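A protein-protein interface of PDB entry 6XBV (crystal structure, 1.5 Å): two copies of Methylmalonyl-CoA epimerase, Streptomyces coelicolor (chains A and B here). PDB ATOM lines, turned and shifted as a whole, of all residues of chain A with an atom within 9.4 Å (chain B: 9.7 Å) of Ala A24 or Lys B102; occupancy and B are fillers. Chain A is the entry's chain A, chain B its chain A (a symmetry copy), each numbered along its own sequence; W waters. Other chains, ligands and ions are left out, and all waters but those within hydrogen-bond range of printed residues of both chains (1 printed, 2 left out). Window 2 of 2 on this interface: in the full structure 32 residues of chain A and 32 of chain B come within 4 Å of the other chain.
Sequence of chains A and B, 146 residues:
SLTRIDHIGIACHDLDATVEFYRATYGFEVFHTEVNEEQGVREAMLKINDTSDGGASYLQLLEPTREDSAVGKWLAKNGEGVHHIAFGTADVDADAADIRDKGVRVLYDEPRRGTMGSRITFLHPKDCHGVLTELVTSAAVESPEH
The backbone carbonyl oxygen (O) of Ala A24 is in hydrogen-bond range of the side-chain amino group (NZ) of Lys B102, at 3.1 Å.
Printed residues of chain B that touch a printed residue of chain A: Leu B2, Ile B99, Lys B102, Leu B123, Asp B127 and His B129.
Hydrophobic or aromatic side chains of chain B within 4 Å of the printed part of chain A: Leu B2, Ile B99, Leu B123 and His B129.
Of the 15 printed residues of chain A, 6 touch a printed residue of chain B.
Among the printed residues, 9 pairs touch across the chains.
Among the printed residues, no Asp or Glu carboxylate lies within 4 Å of a Lys or Arg side-chain nitrogen of the other chain.
No position is printed for both chains.
Of the 9 pairs that touch across the chains among the printed residues, none has its exchanged pair printed and touching as well.
Water W1 lies within hydrogen-bond range of NZ of Lys B102 (2.9 Å) and O of Ala A24 (3.3 Å).
The backbone carbonyl oxygen (O) of Phe A21 is in hydrogen-bond range of the side-chain hydroxyl (OG1) of Thr A25, at 2.8 Å.
The backbone carbonyl oxygen of Tyr A22 sits at hydrogen-bond distance from the backbone NH of Phe A28 (3.4 Å).
The side-chain carboxylate (OD2) of Asp B127 lies within salt-bridge range of the guanidinium group (NE) of Arg B105 (2.9 Å).
Printed residues of chain B within 4 Å of Thr A18: His B129.
Of the printed residues of chain B, Phe A21 touches Asp B127 (3.2 Å) and His B129 (3.8 Å).
Ala A24 touches one residue of chain B.
Of the printed residues of chain B, Phe A28 touches Leu B2.
Asp B95 touches none of the printed residues of chain A.
Of the printed residues of chain A, Lys B102 touches Ala A24 and Thr A25.
No residue of chain A comes within 4 Å of Gly B103.
Printed residues of chain A within 4 Å of Leu B123: Tyr A26.
Of the printed residues of chain A, Asp B127 touches Phe A21 (3.2 Å).
The nearest residue of chain A that does not touch Lys B102 is Tyr A26 (5.3 Å).
The nearest printed residue of chain A that does not touch His B129 is Ala A17 (4.4 Å).
His B129 touches Thr A18 (ND1 to OG1, 3.8 Å).
O of Asp B127 touches CE1 of Phe A21, 3.2 Å away.
CG of Phe A21 touches CD2 of His B129, 3.8 Å away.
Thr A25 touches Ile B99.
Thr A25 touches Lys B102 (O to CE, 3.6 Å).
Tyr A26 touches Leu B2 (CD1 to CD1, 3.3 Å).
Tyr A26 touches Leu B123 (OH to CD1, 3.5 Å).
CE1 of Phe A28 touches O of Leu B2 (3.6 Å).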
ATOM      1  N   ASP A  16     -39.776 -22.714  -5.133  1.00  0.00           N
ATOM      2  CA  ASP A  16     -40.352 -22.842  -3.775  1.00  0.00           C
ATOM      3  C   ASP A  16     -39.574 -23.873  -2.949  1.00  0.00           C
ATOM      4  O   ASP A  16     -39.284 -23.651  -1.714  1.00  0.00           O
ATOM      5  CB  ASP A  16     -41.861 -23.187  -3.854  1.00  0.00           C
ATOM      6  CG  ASP A  16     -42.719 -22.088  -4.446  1.00  0.00           C
ATOM      7  OD1 ASP A  16     -42.275 -20.963  -4.575  1.00  0.00           O
ATOM      8  OD2 ASP A  16     -43.872 -22.414  -4.840  1.00  0.00           O
ATOM      9  N   ALA A  17     -39.190 -24.993  -3.559  1.00  0.00           N
ATOM     10  CA  ALA A  17     -38.479 -26.057  -2.834  1.00  0.00           C
ATOM     11  C   ALA A  17     -37.077 -25.562  -2.424  1.00  0.00           C
ATOM     12  O   ALA A  17     -36.615 -25.820  -1.287  1.00  0.00           O
ATOM     13  CB  ALA A  17     -38.348 -27.274  -3.667  1.00  0.00           C
ATOM     14  N   THR A  18     -36.436 -24.838  -3.329  1.00  0.00           N
ATOM     15  CA  THR A  18     -35.047 -24.373  -3.033  1.00  0.00           C
ATOM     16  C   THR A  18     -35.086 -23.260  -1.981  1.00  0.00           C
ATOM     17  O   THR A  18     -34.245 -23.242  -1.056  1.00  0.00           O
ATOM     18  CB  THR A  18     -34.311 -23.999  -4.325  1.00  0.00           C
ATOM     19  OG1 THR A  18     -34.374 -25.103  -5.256  1.00  0.00           O
ATOM     20  CG2 THR A  18     -32.859 -23.693  -4.059  1.00  0.00           C
ATOM     21  N   VAL A  19     -35.998 -22.310  -2.065  1.00  0.00           N
ATOM     22  CA  VAL A  19     -36.234 -21.301  -1.024  1.00  0.00           C
ATOM     23  C   VAL A  19     -36.410 -21.979   0.340  1.00  0.00           C
ATOM     24  O   VAL A  19     -35.760 -21.566   1.333  1.00  0.00           O
ATOM     25  CB  VAL A  19     -37.428 -20.410  -1.405  1.00  0.00           C
ATOM     26  CG1 VAL A  19     -37.967 -19.716  -0.211  1.00  0.00           C
ATOM     27  CG2 VAL A  19     -37.076 -19.431  -2.500  1.00  0.00           C
ATOM     28  N   GLU A  20     -37.211 -23.047   0.411  1.00  0.00           N
ATOM     29  CA  GLU A  20     -37.428 -23.758   1.694  1.00  0.00           C
ATOM     30  C   GLU A  20     -36.138 -24.435   2.178  1.00  0.00           C
ATOM     31  O   GLU A  20     -35.874 -24.414   3.375  1.00  0.00           O
ATOM     32  CB  GLU A  20     -38.587 -24.749   1.496  1.00  0.00           C
ATOM     33  CG  GLU A  20     -38.818 -25.607   2.731  1.00  0.00           C
ATOM     34  CD  GLU A  20     -39.080 -24.914   4.052  1.00  0.00           C
ATOM     35  OE1 GLU A  20     -39.433 -23.702   4.098  1.00  0.00           O
ATOM     36  OE2 GLU A  20     -38.942 -25.598   5.060  1.00  0.00           O
ATOM     37  N   PHE A  21     -35.353 -24.976   1.259  1.00  0.00           N
ATOM     38  CA  PHE A  21     -34.054 -25.561   1.616  1.00  0.00           C
ATOM     39  C   PHE A  21     -33.177 -24.548   2.356  1.00  0.00           C
ATOM     40  O   PHE A  21     -32.579 -24.791   3.388  1.00  0.00           O
ATOM     41  CB  PHE A  21     -33.343 -26.207   0.417  1.00  0.00           C
ATOM     42  CG  PHE A  21     -31.909 -26.520   0.729  1.00  0.00           C
ATOM     43  CD1 PHE A  21     -31.579 -27.659   1.448  1.00  0.00           C
ATOM     44  CD2 PHE A  21     -30.874 -25.677   0.334  1.00  0.00           C
ATOM     45  CE1 PHE A  21     -30.259 -27.917   1.795  1.00  0.00           C
ATOM     46  CE2 PHE A  21     -29.567 -25.975   0.678  1.00  0.00           C
ATOM     47  CZ  PHE A  21     -29.279 -27.056   1.426  1.00  0.00           C
ATOM     48  N   TYR A  22     -33.073 -23.338   1.741  1.00  0.00           N
ATOM     49  CA  TYR A  22     -32.191 -22.295   2.329  1.00  0.00           C
ATOM     50  C   TYR A  22     -32.790 -21.807   3.680  1.00  0.00           C
ATOM     51  O   TYR A  22     -32.005 -21.494   4.582  1.00  0.00           O
ATOM     52  CB  TYR A  22     -31.957 -21.138   1.313  1.00  0.00           C
ATOM     53  CG  TYR A  22     -30.871 -21.480   0.303  1.00  0.00           C
ATOM     54  CD1 TYR A  22     -31.141 -22.144  -0.868  1.00  0.00           C
ATOM     55  CD2 TYR A  22     -29.549 -21.185   0.592  1.00  0.00           C
ATOM     56  CE1 TYR A  22     -30.134 -22.522  -1.755  1.00  0.00           C
ATOM     57  CE2 TYR A  22     -28.528 -21.637  -0.216  1.00  0.00           C
ATOM     58  CZ  TYR A  22     -28.819 -22.254  -1.418  1.00  0.00           C
ATOM     59  OH  TYR A  22     -27.776 -22.687  -2.197  1.00  0.00           O
ATOM     60  N   ARG A  23     -34.107 -21.707   3.792  1.00  0.00           N
ATOM     61  CA  ARG A  23     -34.728 -21.317   5.087  1.00  0.00           C
ATOM     62  C   ARG A  23     -34.512 -22.388   6.162  1.00  0.00           C
ATOM     63  O   ARG A  23     -34.020 -22.059   7.269  1.00  0.00           O
ATOM     64  CB  ARG A  23     -36.227 -21.061   4.918  1.00  0.00           C
ATOM     65  CG  ARG A  23     -36.888 -20.502   6.172  1.00  0.00           C
ATOM     66  CD  ARG A  23     -38.373 -20.895   6.258  1.00  0.00           C
ATOM     67  NE  ARG A  23     -38.586 -22.334   6.427  1.00  0.00           N
ATOM     68  CZ  ARG A  23     -38.306 -23.030   7.550  1.00  0.00           C
ATOM     69  NH1 ARG A  23     -37.896 -22.421   8.664  1.00  0.00           N
ATOM     70  NH2 ARG A  23     -38.412 -24.343   7.547  1.00  0.00           N
ATOM     71  N   ALA A  24     -34.795 -23.633   5.805  1.00  0.00           N
ATOM     72  CA  ALA A  24     -34.714 -24.720   6.811  1.00  0.00           C
ATOM     73  C   ALA A  24     -33.261 -24.982   7.225  1.00  0.00           C
ATOM     74  O   ALA A  24     -32.949 -25.255   8.427  1.00  0.00           O
ATOM     75  CB  ALA A  24     -35.309 -25.958   6.213  1.00  0.00           C
ATOM     76  N   THR A  25     -32.321 -24.881   6.293  1.00  0.00           N
ATOM     77  CA  THR A  25     -30.941 -25.279   6.545  1.00  0.00           C
ATOM     78  C   THR A  25     -30.163 -24.187   7.258  1.00  0.00           C
ATOM     79  O   THR A  25     -29.297 -24.456   8.126  1.00  0.00           O
ATOM     80  CB  THR A  25     -30.256 -25.781   5.273  1.00  0.00           C
ATOM     81  OG1 THR A  25     -31.096 -26.759   4.670  1.00  0.00           O
ATOM     82  CG2 THR A  25     -28.906 -26.369   5.571  1.00  0.00           C
ATOM     83  N   TYR A  26     -30.318 -22.930   6.785  1.00  0.00           N
ATOM     84  CA  TYR A  26     -29.479 -21.791   7.227  1.00  0.00           C
ATOM     85  C   TYR A  26     -30.263 -20.688   7.953  1.00  0.00           C
ATOM     86  O   TYR A  26     -29.618 -19.743   8.423  1.00  0.00           O
ATOM     87  CB  TYR A  26     -28.782 -21.203   5.996  1.00  0.00           C
ATOM     88  CG  TYR A  26     -28.129 -22.216   5.092  1.00  0.00           C
ATOM     89  CD1 TYR A  26     -27.082 -22.980   5.535  1.00  0.00           C
ATOM     90  CD2 TYR A  26     -28.516 -22.377   3.785  1.00  0.00           C
ATOM     91  CE1 TYR A  26     -26.464 -23.898   4.702  1.00  0.00           C
ATOM     92  CE2 TYR A  26     -27.862 -23.225   2.921  1.00  0.00           C
ATOM     93  CZ  TYR A  26     -26.838 -23.996   3.382  1.00  0.00           C
ATOM     94  OH  TYR A  26     -26.217 -24.833   2.504  1.00  0.00           O
ATOM     95  N   GLY A  27     -31.557 -20.727   7.882  1.00  0.00           N
ATOM     96  CA  GLY A  27     -32.427 -19.665   8.465  1.00  0.00           C
ATOM     97  C   GLY A  27     -32.559 -18.476   7.574  1.00  0.00           C
ATOM     98  O   GLY A  27     -33.065 -17.410   8.051  1.00  0.00           O
ATOM     99  N   PHE A  28     -32.109 -18.535   6.329  1.00  0.00           N
ATOM    100  CA  PHE A  28     -32.228 -17.380   5.423  1.00  0.00           C
ATOM    101  C   PHE A  28     -33.680 -17.182   5.001  1.00  0.00           C
ATOM    102  O   PHE A  28     -34.322 -18.085   4.460  1.00  0.00           O
ATOM    103  CB  PHE A  28     -31.356 -17.568   4.185  1.00  0.00           C
ATOM    104  CG  PHE A  28     -29.884 -17.742   4.422  1.00  0.00           C
ATOM    105  CD1 PHE A  28     -29.221 -17.204   5.527  1.00  0.00           C
ATOM    106  CD2 PHE A  28     -29.128 -18.506   3.553  1.00  0.00           C
ATOM    107  CE1 PHE A  28     -27.857 -17.350   5.667  1.00  0.00           C
ATOM    108  CE2 PHE A  28     -27.778 -18.634   3.671  1.00  0.00           C
ATOM    109  CZ  PHE A  28     -27.134 -18.100   4.748  1.00  0.00           C
ATOM    110  N   GLU A  29     -34.167 -15.935   5.118  1.00  0.00           N
ATOM    111  CA  GLU A  29     -35.549 -15.625   4.740  1.00  0.00           C
ATOM    112  C   GLU A  29     -35.618 -14.895   3.408  1.00  0.00           C
ATOM    113  O   GLU A  29     -34.622 -14.316   2.965  1.00  0.00           O
ATOM    114  CB  GLU A  29     -36.190 -14.734   5.820  1.00  0.00           C
ATOM    115  CG  GLU A  29     -36.244 -15.378   7.209  1.00  0.00           C
ATOM    116  CD  GLU A  29     -37.286 -16.478   7.438  1.00  0.00           C
ATOM    117  OE1 GLU A  29     -38.131 -16.729   6.543  1.00  0.00           O
ATOM    118  OE2 GLU A  29     -37.217 -17.167   8.515  1.00  0.00           O
ATOM    119  N   LEU A  46     -32.596 -13.556  -1.198  1.00  0.00           N
ATOM    120  CA  LEU A  46     -32.387 -13.841   0.243  1.00  0.00           C
ATOM    121  C   LEU A  46     -31.222 -12.974   0.705  1.00  0.00           C
ATOM    122  O   LEU A  46     -30.104 -13.117   0.190  1.00  0.00           O
ATOM    123  CB  LEU A  46     -32.109 -15.329   0.522  1.00  0.00           C
ATOM    124  CG  LEU A  46     -32.850 -16.355  -0.347  1.00  0.00           C
ATOM    125  CD1 LEU A  46     -32.377 -17.763  -0.013  1.00  0.00           C
ATOM    126  CD2 LEU A  46     -34.329 -16.235  -0.168  1.00  0.00           C
ATOM    127  N   LEU B   2     -25.065 -18.256  10.150  1.00  0.00           N
ATOM    128  CA  LEU B   2     -24.311 -17.792   8.959  1.00  0.00           C
ATOM    129  C   LEU B   2     -24.658 -16.313   8.686  1.00  0.00           C
ATOM    130  O   LEU B   2     -25.848 -15.994   8.396  1.00  0.00           O
ATOM    131  CB  LEU B   2     -24.675 -18.678   7.766  1.00  0.00           C
ATOM    132  CG  LEU B   2     -24.439 -20.188   7.911  1.00  0.00           C
ATOM    133  CD1 LEU B   2     -24.752 -20.890   6.606  1.00  0.00           C
ATOM    134  CD2 LEU B   2     -23.041 -20.509   8.358  1.00  0.00           C
ATOM    135  N   ALA B  94     -20.326 -25.231  15.732  1.00  0.00           N
ATOM    136  CA  ALA B  94     -21.737 -25.299  16.173  1.00  0.00           C
ATOM    137  C   ALA B  94     -22.632 -25.344  14.943  1.00  0.00           C
ATOM    138  O   ALA B  94     -23.609 -26.072  14.899  1.00  0.00           O
ATOM    139  CB  ALA B  94     -22.100 -24.100  17.016  1.00  0.00           C
ATOM    140  N   ASP B  95     -22.395 -24.484  13.938  1.00  0.00           N
ATOM    141  CA  ASP B  95     -23.272 -24.442  12.746  1.00  0.00           C
ATOM    142  C   ASP B  95     -23.174 -25.746  11.986  1.00  0.00           C
ATOM    143  O   ASP B  95     -24.211 -26.241  11.489  1.00  0.00           O
ATOM    144  CB  ASP B  95     -22.914 -23.306  11.772  1.00  0.00           C
ATOM    145  CG  ASP B  95     -23.543 -22.009  12.228  1.00  0.00           C
ATOM    146  OD1 ASP B  95     -24.723 -22.032  12.690  1.00  0.00           O
ATOM    147  OD2 ASP B  95     -22.808 -20.998  12.202  1.00  0.00           O
ATOM    148  N   ALA B  96     -21.988 -26.310  11.851  1.00  0.00           N
ATOM    149  CA  ALA B  96     -21.794 -27.590  11.170  1.00  0.00           C
ATOM    150  C   ALA B  96     -22.558 -28.690  11.927  1.00  0.00           C
ATOM    151  O   ALA B  96     -23.218 -29.540  11.261  1.00  0.00           O
ATOM    152  CB  ALA B  96     -20.338 -27.935  11.118  1.00  0.00           C
ATOM    153  N   ALA B  97     -22.505 -28.711  13.256  1.00  0.00           N
ATOM    154  CA  ALA B  97     -23.270 -29.742  14.020  1.00  0.00           C
ATOM    155  C   ALA B  97     -24.773 -29.589  13.791  1.00  0.00           C
ATOM    156  O   ALA B  97     -25.539 -30.586  13.615  1.00  0.00           O
ATOM    157  CB  ALA B  97     -22.959 -29.597  15.484  1.00  0.00           C
ATOM    158  N   ASP B  98     -25.302 -28.364  13.774  1.00  0.00           N
ATOM    159  CA  ASP B  98     -26.735 -28.127  13.599  1.00  0.00           C
ATOM    160  C   ASP B  98     -27.167 -28.592  12.217  1.00  0.00           C
ATOM    161  O   ASP B  98     -28.275 -29.178  12.026  1.00  0.00           O
ATOM    162  CB  ASP B  98     -27.032 -26.656  13.816  1.00  0.00           C
ATOM    163  CG  ASP B  98     -26.990 -26.262  15.276  1.00  0.00           C
ATOM    164  OD1 ASP B  98     -26.915 -27.167  16.152  1.00  0.00           O
ATOM    165  OD2 ASP B  98     -27.033 -25.041  15.511  1.00  0.00           O
ATOM    166  N   ILE B  99     -26.323 -28.344  11.204  1.00  0.00           N
ATOM    167  CA  ILE B  99     -26.631 -28.760   9.825  1.00  0.00           C
ATOM    168  C   ILE B  99     -26.538 -30.314   9.660  1.00  0.00           C
ATOM    169  O   ILE B  99     -27.402 -30.909   8.968  1.00  0.00           O
ATOM    170  CB  ILE B  99     -25.790 -27.953   8.810  1.00  0.00           C
ATOM    171  CG1 ILE B  99     -26.263 -26.503   8.836  1.00  0.00           C
ATOM    172  CG2 ILE B  99     -25.912 -28.528   7.423  1.00  0.00           C
ATOM    173  CD1 ILE B  99     -25.315 -25.505   8.217  1.00  0.00           C
ATOM    174  N   ARG B 100     -25.537 -30.901  10.273  1.00  0.00           N
ATOM    175  CA  ARG B 100     -25.414 -32.405  10.300  1.00  0.00           C
ATOM    176  C   ARG B 100     -26.744 -32.969  10.833  1.00  0.00           C
ATOM    177  O   ARG B 100     -27.238 -33.954  10.253  1.00  0.00           O
ATOM    178  CB  ARG B 100     -24.240 -32.772  11.193  1.00  0.00           C
ATOM    179  CG  ARG B 100     -24.149 -34.272  11.486  1.00  0.00           C
ATOM    180  CD  ARG B 100     -23.308 -34.433  12.747  1.00  0.00           C
ATOM    181  NE  ARG B 100     -24.098 -34.008  13.906  1.00  0.00           N
ATOM    182  CZ  ARG B 100     -23.623 -33.630  15.093  1.00  0.00           C
ATOM    183  NH1 ARG B 100     -22.321 -33.570  15.340  1.00  0.00           N
ATOM    184  NH2 ARG B 100     -24.483 -33.201  15.988  1.00  0.00           N
ATOM    185  N   ASP B 101     -27.300 -32.360  11.865  1.00  0.00           N
ATOM    186  CA  ASP B 101     -28.541 -32.862  12.493  1.00  0.00           C
ATOM    187  C   ASP B 101     -29.760 -32.693  11.627  1.00  0.00           C
ATOM    188  O   ASP B 101     -30.816 -33.288  11.949  1.00  0.00           O
ATOM    189  CB  ASP B 101     -28.739 -32.212  13.824  1.00  0.00           C
ATOM    190  CG  ASP B 101     -27.765 -32.711  14.861  1.00  0.00           C
ATOM    191  OD1 ASP B 101     -27.064 -33.722  14.598  1.00  0.00           O
ATOM    192  OD2 ASP B 101     -27.714 -32.071  15.899  1.00  0.00           O
ATOM    193  N   LYS B 102     -29.686 -31.991  10.490  1.00  0.00           N
ATOM    194  CA  LYS B 102     -30.752 -31.882   9.510  1.00  0.00           C
ATOM    195  C   LYS B 102     -30.592 -32.927   8.421  1.00  0.00           C
ATOM    196  O   LYS B 102     -31.473 -32.998   7.568  1.00  0.00           O
ATOM    197  CB  LYS B 102     -30.763 -30.447   8.946  1.00  0.00           C
ATOM    198  CG  LYS B 102     -31.012 -29.398   9.968  1.00  0.00           C
ATOM    199  CD  LYS B 102     -30.911 -28.057   9.264  1.00  0.00           C
ATOM    200  CE  LYS B 102     -30.810 -26.946  10.251  1.00  0.00           C
ATOM    201  NZ  LYS B 102     -32.088 -26.813  10.928  1.00  0.00           N
ATOM    202  N   GLY B 103     -29.528 -33.749   8.397  1.00  0.00           N
ATOM    203  CA  GLY B 103     -29.328 -34.808   7.396  1.00  0.00           C
ATOM    204  C   GLY B 103     -28.652 -34.359   6.133  1.00  0.00           C
ATOM    205  O   GLY B 103     -28.481 -35.117   5.182  1.00  0.00           O
ATOM    206  N   VAL B 104     -28.146 -33.094   6.122  1.00  0.00           N
ATOM    207  CA  VAL B 104     -27.221 -32.649   5.048  1.00  0.00           C
ATOM    208  C   VAL B 104     -25.823 -33.188   5.327  1.00  0.00           C
ATOM    209  O   VAL B 104     -25.346 -33.062   6.469  1.00  0.00           O
ATOM    210  CB  VAL B 104     -27.191 -31.090   5.014  1.00  0.00           C
ATOM    211  CG1 VAL B 104     -26.113 -30.566   4.043  1.00  0.00           C
ATOM    212  CG2 VAL B 104     -28.544 -30.554   4.643  1.00  0.00           C
ATOM    213  N   ARG B 105     -25.147 -33.795   4.350  1.00  0.00           N
ATOM    214  CA  ARG B 105     -23.826 -34.383   4.553  1.00  0.00           C
ATOM    215  C   ARG B 105     -22.813 -33.277   4.834  1.00  0.00           C
ATOM    216  O   ARG B 105     -22.569 -32.469   3.901  1.00  0.00           O
ATOM    217  CB  ARG B 105     -23.403 -35.243   3.376  1.00  0.00           C
ATOM    218  CG  ARG B 105     -24.081 -36.632   3.420  1.00  0.00           C
ATOM    219  CD  ARG B 105     -23.797 -37.382   2.167  1.00  0.00           C
ATOM    220  NE  ARG B 105     -24.590 -36.873   1.050  1.00  0.00           N
ATOM    221  CZ  ARG B 105     -24.501 -37.249  -0.197  1.00  0.00           C
ATOM    222  NH1 ARG B 105     -23.588 -38.135  -0.580  1.00  0.00           N
ATOM    223  NH2 ARG B 105     -25.323 -36.743  -1.092  1.00  0.00           N
ATOM    224  N   VAL B 106     -22.171 -33.321   5.976  1.00  0.00           N
ATOM    225  CA  VAL B 106     -21.007 -32.478   6.356  1.00  0.00           C
ATOM    226  C   VAL B 106     -19.758 -33.273   6.043  1.00  0.00           C
ATOM    227  O   VAL B 106     -19.606 -34.410   6.625  1.00  0.00           O
ATOM    228  CB  VAL B 106     -21.109 -32.019   7.791  1.00  0.00           C
ATOM    229  CG1 VAL B 106     -19.870 -31.218   8.187  1.00  0.00           C
ATOM    230  CG2 VAL B 106     -22.368 -31.252   8.060  1.00  0.00           C
ATOM    231  N   LEU B 123     -20.354 -28.768   2.815  1.00  0.00           N
ATOM    232  CA  LEU B 123     -21.615 -29.503   2.691  1.00  0.00           C
ATOM    233  C   LEU B 123     -21.668 -30.095   1.310  1.00  0.00           C
ATOM    234  O   LEU B 123     -21.343 -29.440   0.317  1.00  0.00           O
ATOM    235  CB  LEU B 123     -22.796 -28.577   2.930  1.00  0.00           C
ATOM    236  CG  LEU B 123     -22.745 -27.703   4.170  1.00  0.00           C
ATOM    237  CD1 LEU B 123     -23.974 -26.839   4.280  1.00  0.00           C
ATOM    238  CD2 LEU B 123     -22.578 -28.552   5.416  1.00  0.00           C
ATOM    239  N   ASP B 127     -26.649 -32.482  -1.691  1.00  0.00           N
ATOM    240  CA  ASP B 127     -27.614 -32.171  -0.624  1.00  0.00           C
ATOM    241  C   ASP B 127     -27.939 -30.680  -0.571  1.00  0.00           C
ATOM    242  O   ASP B 127     -28.784 -30.285   0.226  1.00  0.00           O
ATOM    243  CB  ASP B 127     -27.065 -32.620   0.711  1.00  0.00           C
ATOM    244  CG  ASP B 127     -26.850 -34.142   0.847  1.00  0.00           C
ATOM    245  OD1 ASP B 127     -27.398 -34.870  -0.037  1.00  0.00           O
ATOM    246  OD2 ASP B 127     -26.226 -34.544   1.816  1.00  0.00           O
ATOM    247  N   HIS B 129     -28.793 -28.690  -3.539  1.00  0.00           N
ATOM    248  CA  HIS B 129     -29.307 -28.286  -4.863  1.00  0.00           C
ATOM    249  C   HIS B 129     -28.153 -27.910  -5.785  1.00  0.00           C
ATOM    250  O   HIS B 129     -28.262 -26.928  -6.562  1.00  0.00           O
ATOM    251  CB  HIS B 129     -30.397 -27.203  -4.698  1.00  0.00           C
ATOM    252  CG  HIS B 129     -31.645 -27.720  -4.069  1.00  0.00           C
ATOM    253  ND1 HIS B 129     -32.558 -28.410  -4.888  1.00  0.00           N
ATOM    254  CD2 HIS B 129     -32.091 -27.795  -2.814  1.00  0.00           C
ATOM    255  CE1 HIS B 129     -33.570 -28.793  -4.102  1.00  0.00           C
ATOM    256  NE2 HIS B 129     -33.367 -28.398  -2.846  1.00  0.00           N
HETATM  257  O   HOH W   1     -34.527 -27.841   9.720  1.00  0.00           O
